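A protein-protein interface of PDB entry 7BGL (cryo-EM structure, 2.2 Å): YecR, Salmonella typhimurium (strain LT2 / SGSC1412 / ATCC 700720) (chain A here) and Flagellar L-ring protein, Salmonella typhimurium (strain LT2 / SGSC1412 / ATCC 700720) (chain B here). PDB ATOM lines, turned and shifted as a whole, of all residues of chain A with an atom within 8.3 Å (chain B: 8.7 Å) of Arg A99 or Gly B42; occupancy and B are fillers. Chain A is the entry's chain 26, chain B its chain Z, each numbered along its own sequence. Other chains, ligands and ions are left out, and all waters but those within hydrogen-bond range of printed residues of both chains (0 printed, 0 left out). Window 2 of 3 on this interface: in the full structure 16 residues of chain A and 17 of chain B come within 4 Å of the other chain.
The backbone carbonyl oxygen (O) of Ala A67 sits at hydrogen-bond distance from the backbone NH (N) of Arg A99 (2.8 Å).
The backbone carbonyl oxygen of Val A70 is in hydrogen-bond range of the backbone NH of Gln A97, 3.1 Å away.
The guanidinium group (NE) of Arg A99 lies close to the side-chain amide oxygen (OE1) of Gln A97, 3.5 Å away.
SG of Cys A61 is disulfide-bonded to SG of Cys A98 (2.0 Å).
Among the printed residues, merely in contact across the chains: Phe A72 with Pro B39, Phe A72 with Ile B40, Phe A72 with Pro B41, Ile A33 with Ile B40, Arg A99 with Gly B42, Gln A97 with Ile B40 and Gln A97 with Gln B56.
Cys A61 touches none of the printed residues of chain B.
Met A64 touches none of the printed residues of chain B.
Printed residues of chain B within 4 Å of Phe A72: Pro B39 (3.2 Å), Ile B40 (3.2 Å) and Pro B41 (3.2 Å).
Of the printed residues of chain B, Gln A97 touches Ile B40 and Gln B56.
Of chain B, only Gly B42 (3.6 Å) comes within 4 Å of Arg A99.
Printed residues of chain A within 4 Å of Pro B39: Phe A72.
Of the printed residues of chain A, Ile B40 touches Ile A33 (3.6 Å), Phe A72 (3.2 Å) and Gln A97 (3.7 Å).
Pro B41 touches one residue of chain A.
Pro B43 touches none of the printed residues of chain A.
The nearest residue of chain B that does not touch Arg A99 is Val B44 (4.1 Å).
The nearest printed residue of chain B that does not touch Phe A72 is Gly B42 (6.5 Å).
Of the 10 printed residues of chain B, 5 touch a printed residue of chain A.
Along chain B the printed residues that touch a printed residue of chain A span positions 39 to 56.
Hydrophobic or aromatic side chains of chain A that line the printed part of chain B: Ile A33 and Phe A72.
Along chain A the printed residues that touch a printed residue of chain B span positions 33 to 99.
Among the printed residues, 7 pairs touch across the chains.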
ATOM      1  N   SER A  31       2.692  16.655  -0.674  1.00  0.00           N
ATOM      2  CA  SER A  31       3.599  17.424  -1.519  1.00  0.00           C
ATOM      3  C   SER A  31       4.078  18.690  -0.815  1.00  0.00           C
ATOM      4  O   SER A  31       4.907  19.413  -1.382  1.00  0.00           O
ATOM      5  CB  SER A  31       2.977  17.804  -2.873  1.00  0.00           C
ATOM      6  OG  SER A  31       1.934  18.748  -2.708  1.00  0.00           O
ATOM      7  N   GLY A  32       3.594  18.983   0.391  1.00  0.00           N
ATOM      8  CA  GLY A  32       4.062  20.134   1.140  1.00  0.00           C
ATOM      9  C   GLY A  32       3.902  21.446   0.401  1.00  0.00           C
ATOM     10  O   GLY A  32       4.884  22.163   0.180  1.00  0.00           O
ATOM     11  N   ILE A  33       2.672  21.775   0.014  1.00  0.00           N
ATOM     12  CA  ILE A  33       2.396  22.936  -0.824  1.00  0.00           C
ATOM     13  C   ILE A  33       1.589  23.948  -0.023  1.00  0.00           C
ATOM     14  O   ILE A  33       0.554  23.607   0.560  1.00  0.00           O
ATOM     15  CB  ILE A  33       1.651  22.544  -2.112  1.00  0.00           C
ATOM     16  CG1 ILE A  33       2.503  21.591  -2.950  1.00  0.00           C
ATOM     17  CG2 ILE A  33       1.289  23.782  -2.916  1.00  0.00           C
ATOM     18  CD1 ILE A  33       3.822  22.184  -3.392  1.00  0.00           C
ATOM     19  N   ALA A  57       4.338  31.799   4.654  1.00  0.00           N
ATOM     20  CA  ALA A  57       4.624  30.464   4.139  1.00  0.00           C
ATOM     21  C   ALA A  57       5.508  29.681   5.100  1.00  0.00           C
ATOM     22  O   ALA A  57       5.287  28.486   5.326  1.00  0.00           O
ATOM     23  CB  ALA A  57       5.280  30.561   2.761  1.00  0.00           C
ATOM     24  N   CYS A  61       4.566  26.197   6.954  1.00  0.00           N
ATOM     25  CA  CYS A  61       5.429  25.023   6.885  1.00  0.00           C
ATOM     26  C   CYS A  61       5.792  24.532   8.281  1.00  0.00           C
ATOM     27  O   CYS A  61       5.764  23.326   8.550  1.00  0.00           O
ATOM     28  CB  CYS A  61       6.689  25.338   6.079  1.00  0.00           C
ATOM     29  SG  CYS A  61       6.397  25.872   4.371  1.00  0.00           S
ATOM     30  N   GLN A  62       6.129  25.456   9.185  1.00  0.00           N
ATOM     31  CA  GLN A  62       6.450  25.069  10.555  1.00  0.00           C
ATOM     32  C   GLN A  62       5.247  24.442  11.246  1.00  0.00           C
ATOM     33  O   GLN A  62       5.384  23.447  11.967  1.00  0.00           O
ATOM     34  CB  GLN A  62       6.953  26.280  11.338  1.00  0.00           C
ATOM     35  CG  GLN A  62       8.347  26.736  10.940  1.00  0.00           C
ATOM     36  CD  GLN A  62       8.701  28.095  11.511  1.00  0.00           C
ATOM     37  OE1 GLN A  62       8.100  28.548  12.484  1.00  0.00           O
ATOM     38  NE2 GLN A  62       9.683  28.753  10.906  1.00  0.00           N
ATOM     39  N   MET A  64       2.981  22.733   9.798  1.00  0.00           N
ATOM     40  CA  MET A  64       3.053  21.388   9.257  1.00  0.00           C
ATOM     41  C   MET A  64       4.429  20.798   9.568  1.00  0.00           C
ATOM     42  O   MET A  64       5.255  21.414  10.249  1.00  0.00           O
ATOM     43  CB  MET A  64       2.750  21.400   7.757  1.00  0.00           C
ATOM     44  CG  MET A  64       1.275  21.585   7.433  1.00  0.00           C
ATOM     45  SD  MET A  64       0.816  20.909   5.827  1.00  0.00           S
ATOM     46  CE  MET A  64       1.142  22.309   4.761  1.00  0.00           C
ATOM     47  N   GLY A  65       4.684  19.587   9.074  1.00  0.00           N
ATOM     48  CA  GLY A  65       5.933  18.912   9.381  1.00  0.00           C
ATOM     49  C   GLY A  65       7.141  19.435   8.631  1.00  0.00           C
ATOM     50  O   GLY A  65       8.266  19.050   8.967  1.00  0.00           O
ATOM     51  N   TYR A  66       6.940  20.293   7.638  1.00  0.00           N
ATOM     52  CA  TYR A  66       8.032  20.817   6.833  1.00  0.00           C
ATOM     53  C   TYR A  66       8.527  22.139   7.420  1.00  0.00           C
ATOM     54  O   TYR A  66       8.188  22.512   8.546  1.00  0.00           O
ATOM     55  CB  TYR A  66       7.587  20.968   5.380  1.00  0.00           C
ATOM     56  CG  TYR A  66       6.956  19.725   4.798  1.00  0.00           C
ATOM     57  CD1 TYR A  66       5.594  19.487   4.931  1.00  0.00           C
ATOM     58  CD2 TYR A  66       7.720  18.790   4.113  1.00  0.00           C
ATOM     59  CE1 TYR A  66       5.013  18.352   4.399  1.00  0.00           C
ATOM     60  CE2 TYR A  66       7.147  17.653   3.577  1.00  0.00           C
ATOM     61  CZ  TYR A  66       5.794  17.439   3.724  1.00  0.00           C
ATOM     62  OH  TYR A  66       5.220  16.307   3.192  1.00  0.00           O
ATOM     63  N   ALA A  67       9.351  22.855   6.660  1.00  0.00           N
ATOM     64  CA  ALA A  67       9.882  24.150   7.071  1.00  0.00           C
ATOM     65  C   ALA A  67      10.674  24.721   5.900  1.00  0.00           C
ATOM     66  O   ALA A  67      10.880  24.055   4.882  1.00  0.00           O
ATOM     67  CB  ALA A  67      10.757  24.043   8.320  1.00  0.00           C
ATOM     68  N   ASP A  68      11.114  25.969   6.057  1.00  0.00           N
ATOM     69  CA  ASP A  68      11.936  26.647   5.056  1.00  0.00           C
ATOM     70  C   ASP A  68      11.217  26.709   3.706  1.00  0.00           C
ATOM     71  O   ASP A  68      11.644  26.123   2.709  1.00  0.00           O
ATOM     72  CB  ASP A  68      13.303  25.965   4.925  1.00  0.00           C
ATOM     73  CG  ASP A  68      14.231  26.696   3.976  1.00  0.00           C
ATOM     74  OD1 ASP A  68      14.755  27.764   4.358  1.00  0.00           O
ATOM     75  OD2 ASP A  68      14.438  26.203   2.847  1.00  0.00           O
ATOM     76  N   ALA A  69      10.101  27.437   3.694  1.00  0.00           N
ATOM     77  CA  ALA A  69       9.320  27.587   2.475  1.00  0.00           C
ATOM     78  C   ALA A  69      10.123  28.309   1.400  1.00  0.00           C
ATOM     79  O   ALA A  69      10.906  29.219   1.689  1.00  0.00           O
ATOM     80  CB  ALA A  69       8.027  28.348   2.768  1.00  0.00           C
ATOM     81  N   VAL A  70       9.923  27.898   0.150  1.00  0.00           N
ATOM     82  CA  VAL A  70      10.602  28.477  -1.003  1.00  0.00           C
ATOM     83  C   VAL A  70       9.549  28.904  -2.015  1.00  0.00           C
ATOM     84  O   VAL A  70       8.601  28.157  -2.284  1.00  0.00           O
ATOM     85  CB  VAL A  70      11.597  27.486  -1.634  1.00  0.00           C
ATOM     86  CG1 VAL A  70      12.299  28.124  -2.823  1.00  0.00           C
ATOM     87  CG2 VAL A  70      12.607  27.017  -0.599  1.00  0.00           C
ATOM     88  N   SER A  71       9.714  30.106  -2.575  1.00  0.00           N
ATOM     89  CA  SER A  71       8.735  30.622  -3.527  1.00  0.00           C
ATOM     90  C   SER A  71       8.607  29.705  -4.738  1.00  0.00           C
ATOM     91  O   SER A  71       7.498  29.327  -5.130  1.00  0.00           O
ATOM     92  CB  SER A  71       9.122  32.036  -3.962  1.00  0.00           C
ATOM     93  OG  SER A  71       8.952  32.962  -2.904  1.00  0.00           O
ATOM     94  N   PHE A  72       9.730  29.394  -5.384  1.00  0.00           N
ATOM     95  CA  PHE A  72       9.818  28.338  -6.389  1.00  0.00           C
ATOM     96  C   PHE A  72       8.985  28.626  -7.634  1.00  0.00           C
ATOM     97  O   PHE A  72       9.074  27.888  -8.620  1.00  0.00           O
ATOM     98  CB  PHE A  72       9.436  26.978  -5.768  1.00  0.00           C
ATOM     99  CG  PHE A  72       7.977  26.592  -5.926  1.00  0.00           C
ATOM    100  CD1 PHE A  72       7.479  26.128  -7.135  1.00  0.00           C
ATOM    101  CD2 PHE A  72       7.118  26.647  -4.840  1.00  0.00           C
ATOM    102  CE1 PHE A  72       6.151  25.773  -7.267  1.00  0.00           C
ATOM    103  CE2 PHE A  72       5.789  26.291  -4.967  1.00  0.00           C
ATOM    104  CZ  PHE A  72       5.306  25.852  -6.181  1.00  0.00           C
ATOM    105  N   TRP A  96       4.368  28.049  -2.511  1.00  0.00           N
ATOM    106  CA  TRP A  96       5.587  27.746  -1.780  1.00  0.00           C
ATOM    107  C   TRP A  96       5.662  26.246  -1.550  1.00  0.00           C
ATOM    108  O   TRP A  96       4.648  25.601  -1.263  1.00  0.00           O
ATOM    109  CB  TRP A  96       5.640  28.486  -0.434  1.00  0.00           C
ATOM    110  CG  TRP A  96       5.351  29.953  -0.535  1.00  0.00           C
ATOM    111  CD1 TRP A  96       4.137  30.538  -0.761  1.00  0.00           C
ATOM    112  CD2 TRP A  96       6.294  31.023  -0.414  1.00  0.00           C
ATOM    113  NE1 TRP A  96       4.268  31.905  -0.788  1.00  0.00           N
ATOM    114  CE2 TRP A  96       5.583  32.229  -0.576  1.00  0.00           C
ATOM    115  CE3 TRP A  96       7.672  31.080  -0.181  1.00  0.00           C
ATOM    116  CZ2 TRP A  96       6.201  33.475  -0.517  1.00  0.00           C
ATOM    117  CZ3 TRP A  96       8.284  32.317  -0.120  1.00  0.00           C
ATOM    118  CH2 TRP A  96       7.550  33.498  -0.290  1.00  0.00           C
ATOM    119  N   GLN A  97       6.865  25.694  -1.676  1.00  0.00           N
ATOM    120  CA  GLN A  97       7.113  24.271  -1.474  1.00  0.00           C
ATOM    121  C   GLN A  97       7.934  24.110  -0.201  1.00  0.00           C
ATOM    122  O   GLN A  97       9.136  24.391  -0.191  1.00  0.00           O
ATOM    123  CB  GLN A  97       7.831  23.666  -2.678  1.00  0.00           C
ATOM    124  CG  GLN A  97       7.951  22.152  -2.638  1.00  0.00           C
ATOM    125  CD  GLN A  97       9.363  21.689  -2.341  1.00  0.00           C
ATOM    126  OE1 GLN A  97      10.331  22.395  -2.620  1.00  0.00           O
ATOM    127  NE2 GLN A  97       9.487  20.496  -1.773  1.00  0.00           N
ATOM    128  N   CYS A  98       7.283  23.659   0.869  1.00  0.00           N
ATOM    129  CA  CYS A  98       7.981  23.478   2.134  1.00  0.00           C
ATOM    130  C   CYS A  98       9.046  22.397   2.002  1.00  0.00           C
ATOM    131  O   CYS A  98       8.828  21.359   1.371  1.00  0.00           O
ATOM    132  CB  CYS A  98       6.992  23.112   3.242  1.00  0.00           C
ATOM    133  SG  CYS A  98       5.601  24.251   3.440  1.00  0.00           S
ATOM    134  N   ARG A  99      10.205  22.645   2.603  1.00  0.00           N
ATOM    135  CA  ARG A  99      11.318  21.706   2.533  1.00  0.00           C
ATOM    136  C   ARG A  99      12.072  21.639   3.857  1.00  0.00           C
ATOM    137  O   ARG A  99      11.479  21.402   4.909  1.00  0.00           O
ATOM    138  CB  ARG A  99      12.274  22.093   1.402  1.00  0.00           C
ATOM    139  CG  ARG A  99      11.763  21.742   0.015  1.00  0.00           C
ATOM    140  CD  ARG A  99      12.858  21.874  -1.030  1.00  0.00           C
ATOM    141  NE  ARG A  99      13.348  23.243  -1.138  1.00  0.00           N
ATOM    142  CZ  ARG A  99      14.273  23.640  -2.002  1.00  0.00           C
ATOM    143  NH1 ARG A  99      14.828  22.796  -2.857  1.00  0.00           N
ATOM    144  NH2 ARG A  99      14.650  24.916  -2.010  1.00  0.00           N
ATOM    145  N   PRO B  39       4.513  24.516 -11.576  1.00  0.00           N
ATOM    146  CA  PRO B  39       5.208  23.296 -11.153  1.00  0.00           C
ATOM    147  C   PRO B  39       6.277  23.589 -10.112  1.00  0.00           C
ATOM    148  O   PRO B  39       6.925  24.638 -10.129  1.00  0.00           O
ATOM    149  CB  PRO B  39       5.820  22.767 -12.455  1.00  0.00           C
ATOM    150  CG  PRO B  39       5.906  23.958 -13.348  1.00  0.00           C
ATOM    151  CD  PRO B  39       4.725  24.811 -13.002  1.00  0.00           C
ATOM    152  N   ILE B  40       6.455  22.641  -9.197  1.00  0.00           N
ATOM    153  CA  ILE B  40       7.466  22.738  -8.146  1.00  0.00           C
ATOM    154  C   ILE B  40       8.802  22.248  -8.692  1.00  0.00           C
ATOM    155  O   ILE B  40       8.848  21.212  -9.372  1.00  0.00           O
ATOM    156  CB  ILE B  40       7.055  21.938  -6.901  1.00  0.00           C
ATOM    157  CG1 ILE B  40       6.270  20.689  -7.308  1.00  0.00           C
ATOM    158  CG2 ILE B  40       6.237  22.798  -5.955  1.00  0.00           C
ATOM    159  CD1 ILE B  40       5.314  20.198  -6.246  1.00  0.00           C
ATOM    160  N   PRO B  41       9.907  22.949  -8.429  1.00  0.00           N
ATOM    161  CA  PRO B  41      11.208  22.450  -8.905  1.00  0.00           C
ATOM    162  C   PRO B  41      11.549  21.073  -8.366  1.00  0.00           C
ATOM    163  O   PRO B  41      12.199  20.280  -9.060  1.00  0.00           O
ATOM    164  CB  PRO B  41      12.194  23.517  -8.409  1.00  0.00           C
ATOM    165  CG  PRO B  41      11.365  24.740  -8.196  1.00  0.00           C
ATOM    166  CD  PRO B  41      10.024  24.249  -7.749  1.00  0.00           C
ATOM    167  N   GLY B  42      11.129  20.764  -7.143  1.00  0.00           N
ATOM    168  CA  GLY B  42      11.414  19.486  -6.539  1.00  0.00           C
ATOM    169  C   GLY B  42      12.508  19.580  -5.497  1.00  0.00           C
ATOM    170  O   GLY B  42      12.955  20.670  -5.125  1.00  0.00           O
ATOM    171  N   PRO B  43      12.964  18.429  -5.001  1.00  0.00           N
ATOM    172  CA  PRO B  43      14.015  18.424  -3.980  1.00  0.00           C
ATOM    173  C   PRO B  43      15.407  18.360  -4.588  1.00  0.00           C
ATOM    174  O   PRO B  43      15.656  17.669  -5.578  1.00  0.00           O
ATOM    175  CB  PRO B  43      13.705  17.151  -3.180  1.00  0.00           C
ATOM    176  CG  PRO B  43      12.927  16.258  -4.136  1.00  0.00           C
ATOM    177  CD  PRO B  43      12.535  17.066  -5.351  1.00  0.00           C
ATOM    178  N   VAL B  44      16.324  19.099  -3.977  1.00  0.00           N
ATOM    179  CA  VAL B  44      17.713  19.106  -4.451  1.00  0.00           C
ATOM    180  C   VAL B  44      18.308  17.715  -4.270  1.00  0.00           C
ATOM    181  O   VAL B  44      18.011  17.044  -3.264  1.00  0.00           O
ATOM    182  CB  VAL B  44      18.526  20.159  -3.698  1.00  0.00           C
ATOM    183  CG1 VAL B  44      18.694  19.757  -2.242  1.00  0.00           C
ATOM    184  CG2 VAL B  44      19.881  20.356  -4.361  1.00  0.00           C
ATOM    185  N   PRO B  45      19.136  17.238  -5.194  1.00  0.00           N
ATOM    186  CA  PRO B  45      19.680  15.883  -5.065  1.00  0.00           C
ATOM    187  C   PRO B  45      20.575  15.746  -3.845  1.00  0.00           C
ATOM    188  O   PRO B  45      21.239  16.694  -3.418  1.00  0.00           O
ATOM    189  CB  PRO B  45      20.478  15.690  -6.361  1.00  0.00           C
ATOM    190  CG  PRO B  45      20.001  16.763  -7.286  1.00  0.00           C
ATOM    191  CD  PRO B  45      19.598  17.908  -6.419  1.00  0.00           C
ATOM    192  N   SER B  54      14.732  10.019  -4.977  1.00  0.00           N
ATOM    193  CA  SER B  54      13.343   9.824  -4.597  1.00  0.00           C
ATOM    194  C   SER B  54      12.569  11.137  -4.715  1.00  0.00           C
ATOM    195  O   SER B  54      13.132  12.206  -4.964  1.00  0.00           O
ATOM    196  CB  SER B  54      13.248   9.277  -3.173  1.00  0.00           C
ATOM    197  OG  SER B  54      13.402  10.312  -2.218  1.00  0.00           O
ATOM    198  N   ALA B  55      11.253  11.044  -4.532  1.00  0.00           N
ATOM    199  CA  ALA B  55      10.371  12.197  -4.677  1.00  0.00           C
ATOM    200  C   ALA B  55       9.355  12.247  -3.543  1.00  0.00           C
ATOM    201  O   ALA B  55       8.188  12.596  -3.749  1.00  0.00           O
ATOM    202  CB  ALA B  55       9.663  12.182  -6.031  1.00  0.00           C
ATOM    203  N   GLN B  56       9.784  11.907  -2.327  1.00  0.00           N
ATOM    204  CA  GLN B  56       8.916  12.036  -1.162  1.00  0.00           C
ATOM    205  C   GLN B  56       7.638  11.224  -1.337  1.00  0.00           C
ATOM    206  O   GLN B  56       6.566  11.797  -1.566  1.00  0.00           O
ATOM    207  CB  GLN B  56       8.579  13.507  -0.910  1.00  0.00           C
ATOM    208  CG  GLN B  56       9.796  14.408  -0.776  1.00  0.00           C
ATOM    209  CD  GLN B  56       9.564  15.791  -1.348  1.00  0.00           C
ATOM    210  OE1 GLN B  56       8.655  16.000  -2.151  1.00  0.00           O
ATOM    211  NE2 GLN B  56      10.387  16.749  -0.935  1.00  0.00           N
